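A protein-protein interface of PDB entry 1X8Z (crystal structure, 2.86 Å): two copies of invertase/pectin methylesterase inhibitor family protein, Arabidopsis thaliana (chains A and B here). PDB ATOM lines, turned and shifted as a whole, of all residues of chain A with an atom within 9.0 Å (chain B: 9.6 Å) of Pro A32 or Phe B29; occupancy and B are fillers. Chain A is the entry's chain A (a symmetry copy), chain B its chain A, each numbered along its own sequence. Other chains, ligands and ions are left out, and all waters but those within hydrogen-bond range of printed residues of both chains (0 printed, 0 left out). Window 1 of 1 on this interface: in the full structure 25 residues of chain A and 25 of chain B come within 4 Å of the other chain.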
ATOM      1  N   MET A   3       8.146 -16.376   8.210  1.00  0.00           N
ATOM      2  CA  MET A   3       9.382 -16.121   7.407  1.00  0.00           C
ATOM      3  C   MET A   3       9.437 -16.997   6.160  1.00  0.00           C
ATOM      4  O   MET A   3       9.001 -18.152   6.185  1.00  0.00           O
ATOM      5  CB  MET A   3      10.631 -16.381   8.257  1.00  0.00           C
ATOM      6  CG  MET A   3      11.956 -16.214   7.508  1.00  0.00           C
ATOM      7  SD  MET A   3      13.400 -16.507   8.556  1.00  0.00           S
ATOM      8  CE  MET A   3      14.693 -15.930   7.492  1.00  0.00           C
ATOM      9  N   ASP A   4       9.990 -16.449   5.079  1.00  0.00           N
ATOM     10  CA  ASP A   4      10.106 -17.178   3.815  1.00  0.00           C
ATOM     11  C   ASP A   4      10.859 -18.492   4.024  1.00  0.00           C
ATOM     12  O   ASP A   4      12.022 -18.496   4.431  1.00  0.00           O
ATOM     13  CB  ASP A   4      10.847 -16.335   2.767  1.00  0.00           C
ATOM     14  CG  ASP A   4      10.402 -14.880   2.756  1.00  0.00           C
ATOM     15  OD1 ASP A   4       9.179 -14.623   2.687  1.00  0.00           O
ATOM     16  OD2 ASP A   4      11.283 -13.990   2.809  1.00  0.00           O
ATOM     17  N   ASN A  26      12.564 -20.350  12.962  1.00  0.00           N
ATOM     18  CA  ASN A  26      11.152 -20.707  12.855  1.00  0.00           C
ATOM     19  C   ASN A  26      10.420 -20.331  14.130  1.00  0.00           C
ATOM     20  O   ASN A  26       9.278 -19.882  14.091  1.00  0.00           O
ATOM     21  CB  ASN A  26      11.001 -22.205  12.610  1.00  0.00           C
ATOM     22  CG  ASN A  26      10.618 -22.514  11.198  1.00  0.00           C
ATOM     23  OD1 ASN A  26      10.742 -23.647  10.736  1.00  0.00           O
ATOM     24  ND2 ASN A  26      10.134 -21.503  10.494  1.00  0.00           N
ATOM     25  N   PHE A  29      10.479 -16.288  14.158  1.00  0.00           N
ATOM     26  CA  PHE A  29       9.664 -15.572  13.182  1.00  0.00           C
ATOM     27  C   PHE A  29       8.637 -16.512  12.601  1.00  0.00           C
ATOM     28  O   PHE A  29       8.719 -16.906  11.432  1.00  0.00           O
ATOM     29  CB  PHE A  29      10.551 -15.022  12.070  1.00  0.00           C
ATOM     30  CG  PHE A  29      11.676 -14.179  12.571  1.00  0.00           C
ATOM     31  CD1 PHE A  29      11.536 -12.800  12.670  1.00  0.00           C
ATOM     32  CD2 PHE A  29      12.853 -14.770  13.007  1.00  0.00           C
ATOM     33  CE1 PHE A  29      12.548 -12.017  13.199  1.00  0.00           C
ATOM     34  CE2 PHE A  29      13.877 -13.993  13.542  1.00  0.00           C
ATOM     35  CZ  PHE A  29      13.722 -12.610  13.639  1.00  0.00           C
ATOM     36  N   ALA A  30       7.663 -16.864  13.428  1.00  0.00           N
ATOM     37  CA  ALA A  30       6.619 -17.784  13.021  1.00  0.00           C
ATOM     38  C   ALA A  30       5.383 -17.105  12.450  1.00  0.00           C
ATOM     39  O   ALA A  30       5.067 -15.955  12.771  1.00  0.00           O
ATOM     40  CB  ALA A  30       6.230 -18.655  14.191  1.00  0.00           C
ATOM     41  N   SER A  31       4.688 -17.838  11.590  1.00  0.00           N
ATOM     42  CA  SER A  31       3.473 -17.347  10.975  1.00  0.00           C
ATOM     43  C   SER A  31       2.475 -17.100  12.109  1.00  0.00           C
ATOM     44  O   SER A  31       2.270 -17.962  12.966  1.00  0.00           O
ATOM     45  CB  SER A  31       2.946 -18.398   9.995  1.00  0.00           C
ATOM     46  OG  SER A  31       1.586 -18.171   9.666  1.00  0.00           O
ATOM     47  N   PRO A  32       1.847 -15.915  12.129  1.00  0.00           N
ATOM     48  CA  PRO A  32       0.871 -15.544  13.157  1.00  0.00           C
ATOM     49  C   PRO A  32      -0.305 -16.482  13.311  1.00  0.00           C
ATOM     50  O   PRO A  32      -0.744 -17.091  12.334  1.00  0.00           O
ATOM     51  CB  PRO A  32       0.432 -14.143  12.729  1.00  0.00           C
ATOM     52  CG  PRO A  32       0.634 -14.154  11.250  1.00  0.00           C
ATOM     53  CD  PRO A  32       1.969 -14.847  11.124  1.00  0.00           C
ATOM     54  N   ASN A  33      -0.802 -16.603  14.543  1.00  0.00           N
ATOM     55  CA  ASN A  33      -1.964 -17.441  14.816  1.00  0.00           C
ATOM     56  C   ASN A  33      -3.219 -16.546  14.851  1.00  0.00           C
ATOM     57  O   ASN A  33      -3.118 -15.314  14.912  1.00  0.00           O
ATOM     58  CB  ASN A  33      -1.810 -18.190  16.136  1.00  0.00           C
ATOM     59  CG  ASN A  33      -2.109 -17.331  17.319  1.00  0.00           C
ATOM     60  OD1 ASN A  33      -3.149 -16.680  17.376  1.00  0.00           O
ATOM     61  ND2 ASN A  33      -1.205 -17.325  18.290  1.00  0.00           N
ATOM     62  N   LEU A  34      -4.400 -17.158  14.819  1.00  0.00           N
ATOM     63  CA  LEU A  34      -5.638 -16.383  14.790  1.00  0.00           C
ATOM     64  C   LEU A  34      -5.810 -15.341  15.898  1.00  0.00           C
ATOM     65  O   LEU A  34      -6.178 -14.205  15.603  1.00  0.00           O
ATOM     66  CB  LEU A  34      -6.837 -17.331  14.740  1.00  0.00           C
ATOM     67  CG  LEU A  34      -6.895 -18.150  13.441  1.00  0.00           C
ATOM     68  CD1 LEU A  34      -8.144 -19.022  13.434  1.00  0.00           C
ATOM     69  CD2 LEU A  34      -6.882 -17.216  12.237  1.00  0.00           C
ATOM     70  N   GLN A  35      -5.547 -15.717  17.153  1.00  0.00           N
ATOM     71  CA  GLN A  35      -5.654 -14.792  18.286  1.00  0.00           C
ATOM     72  C   GLN A  35      -4.801 -13.563  17.983  1.00  0.00           C
ATOM     73  O   GLN A  35      -5.280 -12.435  17.986  1.00  0.00           O
ATOM     74  CB  GLN A  35      -5.141 -15.443  19.580  1.00  0.00           C
ATOM     75  CG  GLN A  35      -5.978 -16.594  20.132  1.00  0.00           C
ATOM     76  CD  GLN A  35      -7.182 -16.136  20.976  1.00  0.00           C
ATOM     77  OE1 GLN A  35      -8.193 -16.845  21.069  1.00  0.00           O
ATOM     78  NE2 GLN A  35      -7.069 -14.962  21.603  1.00  0.00           N
ATOM     79  N   ALA A  36      -3.523 -13.803  17.711  1.00  0.00           N
ATOM     80  CA  ALA A  36      -2.581 -12.736  17.405  1.00  0.00           C
ATOM     81  C   ALA A  36      -3.074 -11.809  16.297  1.00  0.00           C
ATOM     82  O   ALA A  36      -2.897 -10.596  16.379  1.00  0.00           O
ATOM     83  CB  ALA A  36      -1.255 -13.328  17.015  1.00  0.00           C
ATOM     84  N   LEU A  37      -3.684 -12.369  15.258  1.00  0.00           N
ATOM     85  CA  LEU A  37      -4.178 -11.540  14.162  1.00  0.00           C
ATOM     86  C   LEU A  37      -5.312 -10.670  14.641  1.00  0.00           C
ATOM     87  O   LEU A  37      -5.401  -9.493  14.295  1.00  0.00           O
ATOM     88  CB  LEU A  37      -4.665 -12.405  13.009  1.00  0.00           C
ATOM     89  CG  LEU A  37      -3.565 -13.038  12.165  1.00  0.00           C
ATOM     90  CD1 LEU A  37      -4.201 -13.969  11.130  1.00  0.00           C
ATOM     91  CD2 LEU A  37      -2.752 -11.946  11.494  1.00  0.00           C
ATOM     92  N   ALA A  38      -6.176 -11.263  15.450  1.00  0.00           N
ATOM     93  CA  ALA A  38      -7.311 -10.548  15.990  1.00  0.00           C
ATOM     94  C   ALA A  38      -6.842  -9.478  16.975  1.00  0.00           C
ATOM     95  O   ALA A  38      -7.302  -8.337  16.929  1.00  0.00           O
ATOM     96  CB  ALA A  38      -8.252 -11.522  16.678  1.00  0.00           C
ATOM     97  N   LYS A  39      -5.917  -9.851  17.856  1.00  0.00           N
ATOM     98  CA  LYS A  39      -5.391  -8.940  18.863  1.00  0.00           C
ATOM     99  C   LYS A  39      -4.766  -7.712  18.231  1.00  0.00           C
ATOM    100  O   LYS A  39      -4.950  -6.601  18.719  1.00  0.00           O
ATOM    101  CB  LYS A  39      -4.368  -9.662  19.736  1.00  0.00           C
ATOM    102  CG  LYS A  39      -3.944  -8.909  20.988  1.00  0.00           C
ATOM    103  CD  LYS A  39      -2.895  -7.844  20.722  1.00  0.00           C
ATOM    104  CE  LYS A  39      -2.434  -7.273  22.040  1.00  0.00           C
ATOM    105  NZ  LYS A  39      -1.346  -6.266  21.945  1.00  0.00           N
ATOM    106  N   THR A  40      -4.023  -7.902  17.148  1.00  0.00           N
ATOM    107  CA  THR A  40      -3.413  -6.760  16.469  1.00  0.00           C
ATOM    108  C   THR A  40      -4.545  -5.878  15.909  1.00  0.00           C
ATOM    109  O   THR A  40      -4.640  -4.683  16.219  1.00  0.00           O
ATOM    110  CB  THR A  40      -2.475  -7.223  15.314  1.00  0.00           C
ATOM    111  OG1 THR A  40      -1.355  -7.929  15.862  1.00  0.00           O
ATOM    112  CG2 THR A  40      -1.968  -6.037  14.509  1.00  0.00           C
ATOM    113  N   THR A  41      -5.423  -6.479  15.112  1.00  0.00           N
ATOM    114  CA  THR A  41      -6.521  -5.737  14.515  1.00  0.00           C
ATOM    115  C   THR A  41      -7.309  -4.902  15.529  1.00  0.00           C
ATOM    116  O   THR A  41      -7.615  -3.740  15.261  1.00  0.00           O
ATOM    117  CB  THR A  41      -7.446  -6.688  13.757  1.00  0.00           C
ATOM    118  OG1 THR A  41      -6.646  -7.524  12.916  1.00  0.00           O
ATOM    119  CG2 THR A  41      -8.415  -5.919  12.873  1.00  0.00           C
ATOM    120  N   LEU A  42      -7.632  -5.471  16.689  1.00  0.00           N
ATOM    121  CA  LEU A  42      -8.354  -4.702  17.711  1.00  0.00           C
ATOM    122  C   LEU A  42      -7.496  -3.554  18.251  1.00  0.00           C
ATOM    123  O   LEU A  42      -8.007  -2.476  18.523  1.00  0.00           O
ATOM    124  CB  LEU A  42      -8.794  -5.586  18.880  1.00  0.00           C
ATOM    125  CG  LEU A  42      -9.933  -6.560  18.575  1.00  0.00           C
ATOM    126  CD1 LEU A  42     -10.330  -7.330  19.828  1.00  0.00           C
ATOM    127  CD2 LEU A  42     -11.116  -5.787  18.065  1.00  0.00           C
ATOM    128  N   SER A  44      -5.322  -1.797  16.648  1.00  0.00           N
ATOM    129  CA  SER A  44      -5.412  -0.743  15.637  1.00  0.00           C
ATOM    130  C   SER A  44      -6.745  -0.001  15.684  1.00  0.00           C
ATOM    131  O   SER A  44      -6.797   1.224  15.638  1.00  0.00           O
ATOM    132  CB  SER A  44      -5.188  -1.328  14.232  1.00  0.00           C
ATOM    133  OG  SER A  44      -3.803  -1.577  13.967  1.00  0.00           O
ATOM    134  N   ILE A 142     -12.356  -6.930   9.263  1.00  0.00           N
ATOM    135  CA  ILE A 142     -11.325  -7.951   9.402  1.00  0.00           C
ATOM    136  C   ILE A 142     -11.583  -8.730  10.697  1.00  0.00           C
ATOM    137  O   ILE A 142     -11.648  -9.960  10.692  1.00  0.00           O
ATOM    138  CB  ILE A 142      -9.925  -7.297   9.464  1.00  0.00           C
ATOM    139  CG1 ILE A 142      -9.711  -6.472   8.198  1.00  0.00           C
ATOM    140  CG2 ILE A 142      -8.848  -8.352   9.626  1.00  0.00           C
ATOM    141  CD1 ILE A 142      -8.393  -5.770   8.128  1.00  0.00           C
ATOM    142  N   ILE A 146     -12.008 -12.888  11.254  1.00  0.00           N
ATOM    143  CA  ILE A 146     -11.150 -13.598  12.200  1.00  0.00           C
ATOM    144  C   ILE A 146     -11.933 -14.209  13.361  1.00  0.00           C
ATOM    145  O   ILE A 146     -11.852 -15.408  13.585  1.00  0.00           O
ATOM    146  CB  ILE A 146     -10.022 -12.664  12.752  1.00  0.00           C
ATOM    147  CG1 ILE A 146      -9.090 -12.262  11.607  1.00  0.00           C
ATOM    148  CG2 ILE A 146      -9.190 -13.388  13.790  1.00  0.00           C
ATOM    149  CD1 ILE A 146      -8.033 -11.256  11.967  1.00  0.00           C
ATOM    150  N   MET B   3       3.726 -13.783   6.939  1.00  0.00           N
ATOM    151  CA  MET B   3       2.418 -14.502   7.045  1.00  0.00           C
ATOM    152  C   MET B   3       2.105 -15.297   5.782  1.00  0.00           C
ATOM    153  O   MET B   3       2.429 -14.865   4.673  1.00  0.00           O
ATOM    154  CB  MET B   3       1.283 -13.504   7.303  1.00  0.00           C
ATOM    155  CG  MET B   3      -0.113 -14.130   7.363  1.00  0.00           C
ATOM    156  SD  MET B   3      -1.416 -12.919   7.692  1.00  0.00           S
ATOM    157  CE  MET B   3      -2.786 -13.997   8.004  1.00  0.00           C
ATOM    158  N   ASP B   4       1.459 -16.449   5.957  1.00  0.00           N
ATOM    159  CA  ASP B   4       1.096 -17.311   4.831  1.00  0.00           C
ATOM    160  C   ASP B   4       0.260 -16.536   3.812  1.00  0.00           C
ATOM    161  O   ASP B   4      -0.828 -16.053   4.127  1.00  0.00           O
ATOM    162  CB  ASP B   4       0.297 -18.530   5.314  1.00  0.00           C
ATOM    163  CG  ASP B   4       0.871 -19.149   6.580  1.00  0.00           C
ATOM    164  OD1 ASP B   4       2.091 -19.428   6.616  1.00  0.00           O
ATOM    165  OD2 ASP B   4       0.094 -19.365   7.540  1.00  0.00           O
ATOM    166  N   SER B   5       0.775 -16.418   2.592  1.00  0.00           N
ATOM    167  CA  SER B   5       0.071 -15.703   1.530  1.00  0.00           C
ATOM    168  C   SER B   5      -1.305 -16.335   1.339  1.00  0.00           C
ATOM    169  O   SER B   5      -2.253 -15.687   0.896  1.00  0.00           O
ATOM    170  CB  SER B   5       0.869 -15.793   0.227  1.00  0.00           C
ATOM    171  OG  SER B   5       2.229 -15.450   0.437  1.00  0.00           O
ATOM    172  N   GLU B   7      -3.405 -18.058   3.827  1.00  0.00           N
ATOM    173  CA  GLU B   7      -4.301 -17.642   4.897  1.00  0.00           C
ATOM    174  C   GLU B   7      -4.648 -16.164   4.742  1.00  0.00           C
ATOM    175  O   GLU B   7      -5.799 -15.764   4.921  1.00  0.00           O
ATOM    176  CB  GLU B   7      -3.616 -17.885   6.250  1.00  0.00           C
ATOM    177  CG  GLU B   7      -4.499 -17.740   7.491  1.00  0.00           C
ATOM    178  CD  GLU B   7      -3.708 -17.894   8.789  1.00  0.00           C
ATOM    179  OE1 GLU B   7      -4.333 -17.966   9.871  1.00  0.00           O
ATOM    180  OE2 GLU B   7      -2.459 -17.940   8.727  1.00  0.00           O
ATOM    181  N   MET B   8      -3.646 -15.358   4.398  1.00  0.00           N
ATOM    182  CA  MET B   8      -3.844 -13.924   4.230  1.00  0.00           C
ATOM    183  C   MET B   8      -4.941 -13.661   3.204  1.00  0.00           C
ATOM    184  O   MET B   8      -5.808 -12.812   3.407  1.00  0.00           O
ATOM    185  CB  MET B   8      -2.535 -13.255   3.796  1.00  0.00           C
ATOM    186  CG  MET B   8      -2.498 -11.752   4.053  1.00  0.00           C
ATOM    187  SD  MET B   8      -0.908 -10.968   3.665  1.00  0.00           S
ATOM    188  CE  MET B   8      -0.045 -11.126   5.235  1.00  0.00           C
ATOM    189  N   ILE B  11      -8.374 -14.845   4.316  1.00  0.00           N
ATOM    190  CA  ILE B  11      -9.014 -13.931   5.253  1.00  0.00           C
ATOM    191  C   ILE B  11      -9.559 -12.681   4.580  1.00  0.00           C
ATOM    192  O   ILE B  11     -10.736 -12.341   4.736  1.00  0.00           O
ATOM    193  CB  ILE B  11      -8.026 -13.537   6.368  1.00  0.00           C
ATOM    194  CG1 ILE B  11      -7.738 -14.767   7.233  1.00  0.00           C
ATOM    195  CG2 ILE B  11      -8.590 -12.396   7.205  1.00  0.00           C
ATOM    196  CD1 ILE B  11      -6.879 -14.498   8.443  1.00  0.00           C
ATOM    197  N   CYS B  21      -7.539  -4.737   3.802  1.00  0.00           N
ATOM    198  CA  CYS B  21      -7.226  -5.858   4.679  1.00  0.00           C
ATOM    199  C   CYS B  21      -5.870  -6.478   4.355  1.00  0.00           C
ATOM    200  O   CYS B  21      -5.076  -6.744   5.256  1.00  0.00           O
ATOM    201  CB  CYS B  21      -8.329  -6.907   4.561  1.00  0.00           C
ATOM    202  SG  CYS B  21      -7.945  -8.571   5.196  1.00  0.00           S
ATOM    203  N   LEU B  22      -5.609  -6.711   3.072  1.00  0.00           N
ATOM    204  CA  LEU B  22      -4.336  -7.288   2.647  1.00  0.00           C
ATOM    205  C   LEU B  22      -3.172  -6.362   2.938  1.00  0.00           C
ATOM    206  O   LEU B  22      -2.109  -6.813   3.358  1.00  0.00           O
ATOM    207  CB  LEU B  22      -4.336  -7.592   1.152  1.00  0.00           C
ATOM    208  CG  LEU B  22      -4.865  -8.943   0.682  1.00  0.00           C
ATOM    209  CD1 LEU B  22      -4.780  -8.981  -0.835  1.00  0.00           C
ATOM    210  CD2 LEU B  22      -4.055 -10.078   1.310  1.00  0.00           C
ATOM    211  N   LYS B  23      -3.362  -5.069   2.695  1.00  0.00           N
ATOM    212  CA  LYS B  23      -2.301  -4.104   2.950  1.00  0.00           C
ATOM    213  C   LYS B  23      -2.025  -4.027   4.451  1.00  0.00           C
ATOM    214  O   LYS B  23      -0.875  -3.908   4.890  1.00  0.00           O
ATOM    215  CB  LYS B  23      -2.694  -2.722   2.415  1.00  0.00           C
ATOM    216  CG  LYS B  23      -1.590  -1.674   2.540  1.00  0.00           C
ATOM    217  CD  LYS B  23      -1.962  -0.390   1.807  1.00  0.00           C
ATOM    218  CE  LYS B  23      -0.808   0.596   1.809  1.00  0.00           C
ATOM    219  NZ  LYS B  23      -0.348   0.859   3.200  1.00  0.00           N
ATOM    220  N   PHE B  24      -3.092  -4.113   5.238  1.00  0.00           N
ATOM    221  CA  PHE B  24      -2.957  -4.050   6.677  1.00  0.00           C
ATOM    222  C   PHE B  24      -2.198  -5.248   7.236  1.00  0.00           C
ATOM    223  O   PHE B  24      -1.207  -5.091   7.951  1.00  0.00           O
ATOM    224  CB  PHE B  24      -4.331  -3.974   7.340  1.00  0.00           C
ATOM    225  CG  PHE B  24      -4.265  -3.926   8.837  1.00  0.00           C
ATOM    226  CD1 PHE B  24      -3.697  -2.832   9.483  1.00  0.00           C
ATOM    227  CD2 PHE B  24      -4.711  -5.001   9.600  1.00  0.00           C
ATOM    228  CE1 PHE B  24      -3.570  -2.812  10.860  1.00  0.00           C
ATOM    229  CE2 PHE B  24      -4.589  -4.993  10.979  1.00  0.00           C
ATOM    230  CZ  PHE B  24      -4.019  -3.899  11.612  1.00  0.00           C
ATOM    231  N   LEU B  25      -2.668  -6.447   6.916  1.00  0.00           N
ATOM    232  CA  LEU B  25      -2.035  -7.656   7.421  1.00  0.00           C
ATOM    233  C   LEU B  25      -0.594  -7.829   6.959  1.00  0.00           C
ATOM    234  O   LEU B  25       0.262  -8.279   7.734  1.00  0.00           O
ATOM    235  CB  LEU B  25      -2.876  -8.876   7.046  1.00  0.00           C
ATOM    236  CG  LEU B  25      -3.806  -9.434   8.138  1.00  0.00           C
ATOM    237  CD1 LEU B  25      -4.121  -8.398   9.206  1.00  0.00           C
ATOM    238  CD2 LEU B  25      -5.077  -9.928   7.479  1.00  0.00           C
ATOM    239  N   ASN B  26      -0.330  -7.464   5.708  1.00  0.00           N
ATOM    240  CA  ASN B  26       1.013  -7.555   5.141  1.00  0.00           C
ATOM    241  C   ASN B  26       1.950  -6.604   5.860  1.00  0.00           C
ATOM    242  O   ASN B  26       3.112  -6.922   6.095  1.00  0.00           O
ATOM    243  CB  ASN B  26       0.985  -7.210   3.656  1.00  0.00           C
ATOM    244  CG  ASN B  26       1.134  -8.420   2.788  1.00  0.00           C
ATOM    245  OD1 ASN B  26       0.839  -8.389   1.595  1.00  0.00           O
ATOM    246  ND2 ASN B  26       1.607  -9.504   3.381  1.00  0.00           N
ATOM    247  N   THR B  27       1.436  -5.426   6.196  1.00  0.00           N
ATOM    248  CA  THR B  27       2.216  -4.430   6.913  1.00  0.00           C
ATOM    249  C   THR B  27       2.482  -4.923   8.325  1.00  0.00           C
ATOM    250  O   THR B  27       3.591  -4.826   8.839  1.00  0.00           O
ATOM    251  CB  THR B  27       1.450  -3.119   7.032  1.00  0.00           C
ATOM    252  OG1 THR B  27       1.248  -2.564   5.728  1.00  0.00           O
ATOM    253  CG2 THR B  27       2.210  -2.142   7.913  1.00  0.00           C
ATOM    254  N   LYS B  28       1.441  -5.453   8.946  1.00  0.00           N
ATOM    255  CA  LYS B  28       1.519  -5.946  10.305  1.00  0.00           C
ATOM    256  C   LYS B  28       2.326  -7.219  10.523  1.00  0.00           C
ATOM    257  O   LYS B  28       2.989  -7.361  11.542  1.00  0.00           O
ATOM    258  CB  LYS B  28       0.100  -6.133  10.844  1.00  0.00           C
ATOM    259  CG  LYS B  28      -0.582  -4.822  11.170  1.00  0.00           C
ATOM    260  CD  LYS B  28       0.175  -4.138  12.296  1.00  0.00           C
ATOM    261  CE  LYS B  28      -0.465  -2.831  12.729  1.00  0.00           C
ATOM    262  NZ  LYS B  28       0.266  -2.245  13.900  1.00  0.00           N
ATOM    263  N   PHE B  29       2.277  -8.149   9.583  1.00  0.00           N
ATOM    264  CA  PHE B  29       3.010  -9.400   9.757  1.00  0.00           C
ATOM    265  C   PHE B  29       3.851  -9.662   8.532  1.00  0.00           C
ATOM    266  O   PHE B  29       3.567 -10.571   7.744  1.00  0.00           O
ATOM    267  CB  PHE B  29       2.030 -10.549   9.969  1.00  0.00           C
ATOM    268  CG  PHE B  29       1.072 -10.313  11.088  1.00  0.00           C
ATOM    269  CD1 PHE B  29       1.354 -10.773  12.369  1.00  0.00           C
ATOM    270  CD2 PHE B  29      -0.083  -9.572  10.877  1.00  0.00           C
ATOM    271  CE1 PHE B  29       0.505 -10.499  13.427  1.00  0.00           C
ATOM    272  CE2 PHE B  29      -0.943  -9.288  11.934  1.00  0.00           C
ATOM    273  CZ  PHE B  29      -0.645  -9.753  13.216  1.00  0.00           C
ATOM    274  N   ALA B  30       4.895  -8.859   8.383  1.00  0.00           N
ATOM    275  CA  ALA B  30       5.779  -8.971   7.239  1.00  0.00           C
ATOM    276  C   ALA B  30       6.980  -9.875   7.472  1.00  0.00           C
ATOM    277  O   ALA B  30       7.445 -10.060   8.601  1.00  0.00           O
ATOM    278  CB  ALA B  30       6.246  -7.596   6.825  1.00  0.00           C
ATOM    279  N   SER B  31       7.474 -10.443   6.378  1.00  0.00           N
ATOM    280  CA  SER B  31       8.630 -11.312   6.426  1.00  0.00           C
ATOM    281  C   SER B  31       9.798 -10.464   6.936  1.00  0.00           C
ATOM    282  O   SER B  31      10.040  -9.362   6.439  1.00  0.00           O
ATOM    283  CB  SER B  31       8.912 -11.849   5.020  1.00  0.00           C
ATOM    284  OG  SER B  31      10.227 -12.368   4.912  1.00  0.00           O
ATOM    285  N   PRO B  32      10.531 -10.967   7.940  1.00  0.00           N
ATOM    286  CA  PRO B  32      11.674 -10.262   8.528  1.00  0.00           C
ATOM    287  C   PRO B  32      12.766  -9.866   7.560  1.00  0.00           C
ATOM    288  O   PRO B  32      13.003 -10.565   6.573  1.00  0.00           O
ATOM    289  CB  PRO B  32      12.178 -11.242   9.588  1.00  0.00           C
ATOM    290  CG  PRO B  32      11.768 -12.574   9.052  1.00  0.00           C
ATOM    291  CD  PRO B  32      10.369 -12.292   8.559  1.00  0.00           C
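Of the 20 printed residues of chain A, 12 touch a printed residue of chain B. Hydrophobic or aromatic side chains of chain A within 4 Å of the printed part of chain B: Met A3, Phe A29, Pro A32, Leu A34, Leu A37 and Ile A142. Of the 18 printed residues of chain B, 10 touch a printed residue of chain A. Printed residues of chain B that touch a printed residue of chain A: Met B3, Asp B4, Glu B7, Ile B11, Cys B21, Phe B24, Lys B28, Phe B29, Ser B31 and Pro B32. Hydrophobic or aromatic side chains of chain B within 4 Å of the printed part of chain A: Met B3, Ile B11, Phe B24, Phe B29 and Pro B32.
Pro A32 touches just these residues of chain B: Met B3 and Phe B29. No residue of chain B comes within 4 Å of Asn A33. No residue of chain A comes within 4 Å of Ala B30. Printed residues of chain A within 4 Å of Pro B32: Met A3 (3.96 Å) and Phe A29 (3.5 Å). Printed residues of chain A within 4 Å of Ile B11: Leu A37. Of the printed residues of chain A, Lys B28 touches Thr A40 and Ser A44. Of the printed residues of chain A, Phe B24 touches Thr A41 (3.8 Å) and Ser A44 (3.3 Å). Ala A30 touches none of the printed residues of chain B. The nearest residue of chain A that does not touch Phe B29 is Thr A41 (6.0 Å). The nearest printed residue of chain A that does not touch Ser B31 is Met A3 (4.6 Å).
The side-chain hydroxyl (OG) of Ser B31 is in hydrogen-bond range of the side-chain carboxylate (OD2) of Asp A4 (2.9 Å). The side-chain carboxylate (OD2) of Asp B4 is in hydrogen-bond range of the side-chain hydroxyl (OG) of Ser A31.
Among the printed residues, pairs that only touch across the chains: Leu A37 with Phe B29, Thr A40 with Phe B29, Ser A44 with Phe B24, Leu A37 with Met B3, Pro A32 with Phe B29, Phe A29 with Pro B32, Leu A34 with Glu B7, Thr A40 with Lys B28, Ile A142 with Cys B21, Ser A44 with Lys B28, Thr A41 with Phe B24, Leu A37 with Ile B11, Pro A32 with Met B3, Met A3 with Pro B32 and Ala A36 with Phe B29.
O of Leu A37 sits at hydrogen-bond distance from OG1 of Thr A41 (2.7 Å). N of Met A3 sits at hydrogen-bond distance from O of Phe A29. The backbone NH of Met B3 is in hydrogen-bond range of the backbone carbonyl oxygen of Phe B29, at 3.3 Å. OG1 of Thr A40 lies within hydrogen-bond range of O of Ala A36 (3.1 Å). The backbone NH of Ala A36 is in hydrogen-bond range of the side-chain amide oxygen of Asn A33.
Met A3 touches Pro B32, and with the chains exchanged Pro A32 touches Met B3. Asp A4 touches Ser B31, and with the chains exchanged Ser A31 touches Asp B4. Phe A29 touches Pro B32, and with the chains exchanged Pro A32 touches Phe B29. 7 positions are printed for both chains.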
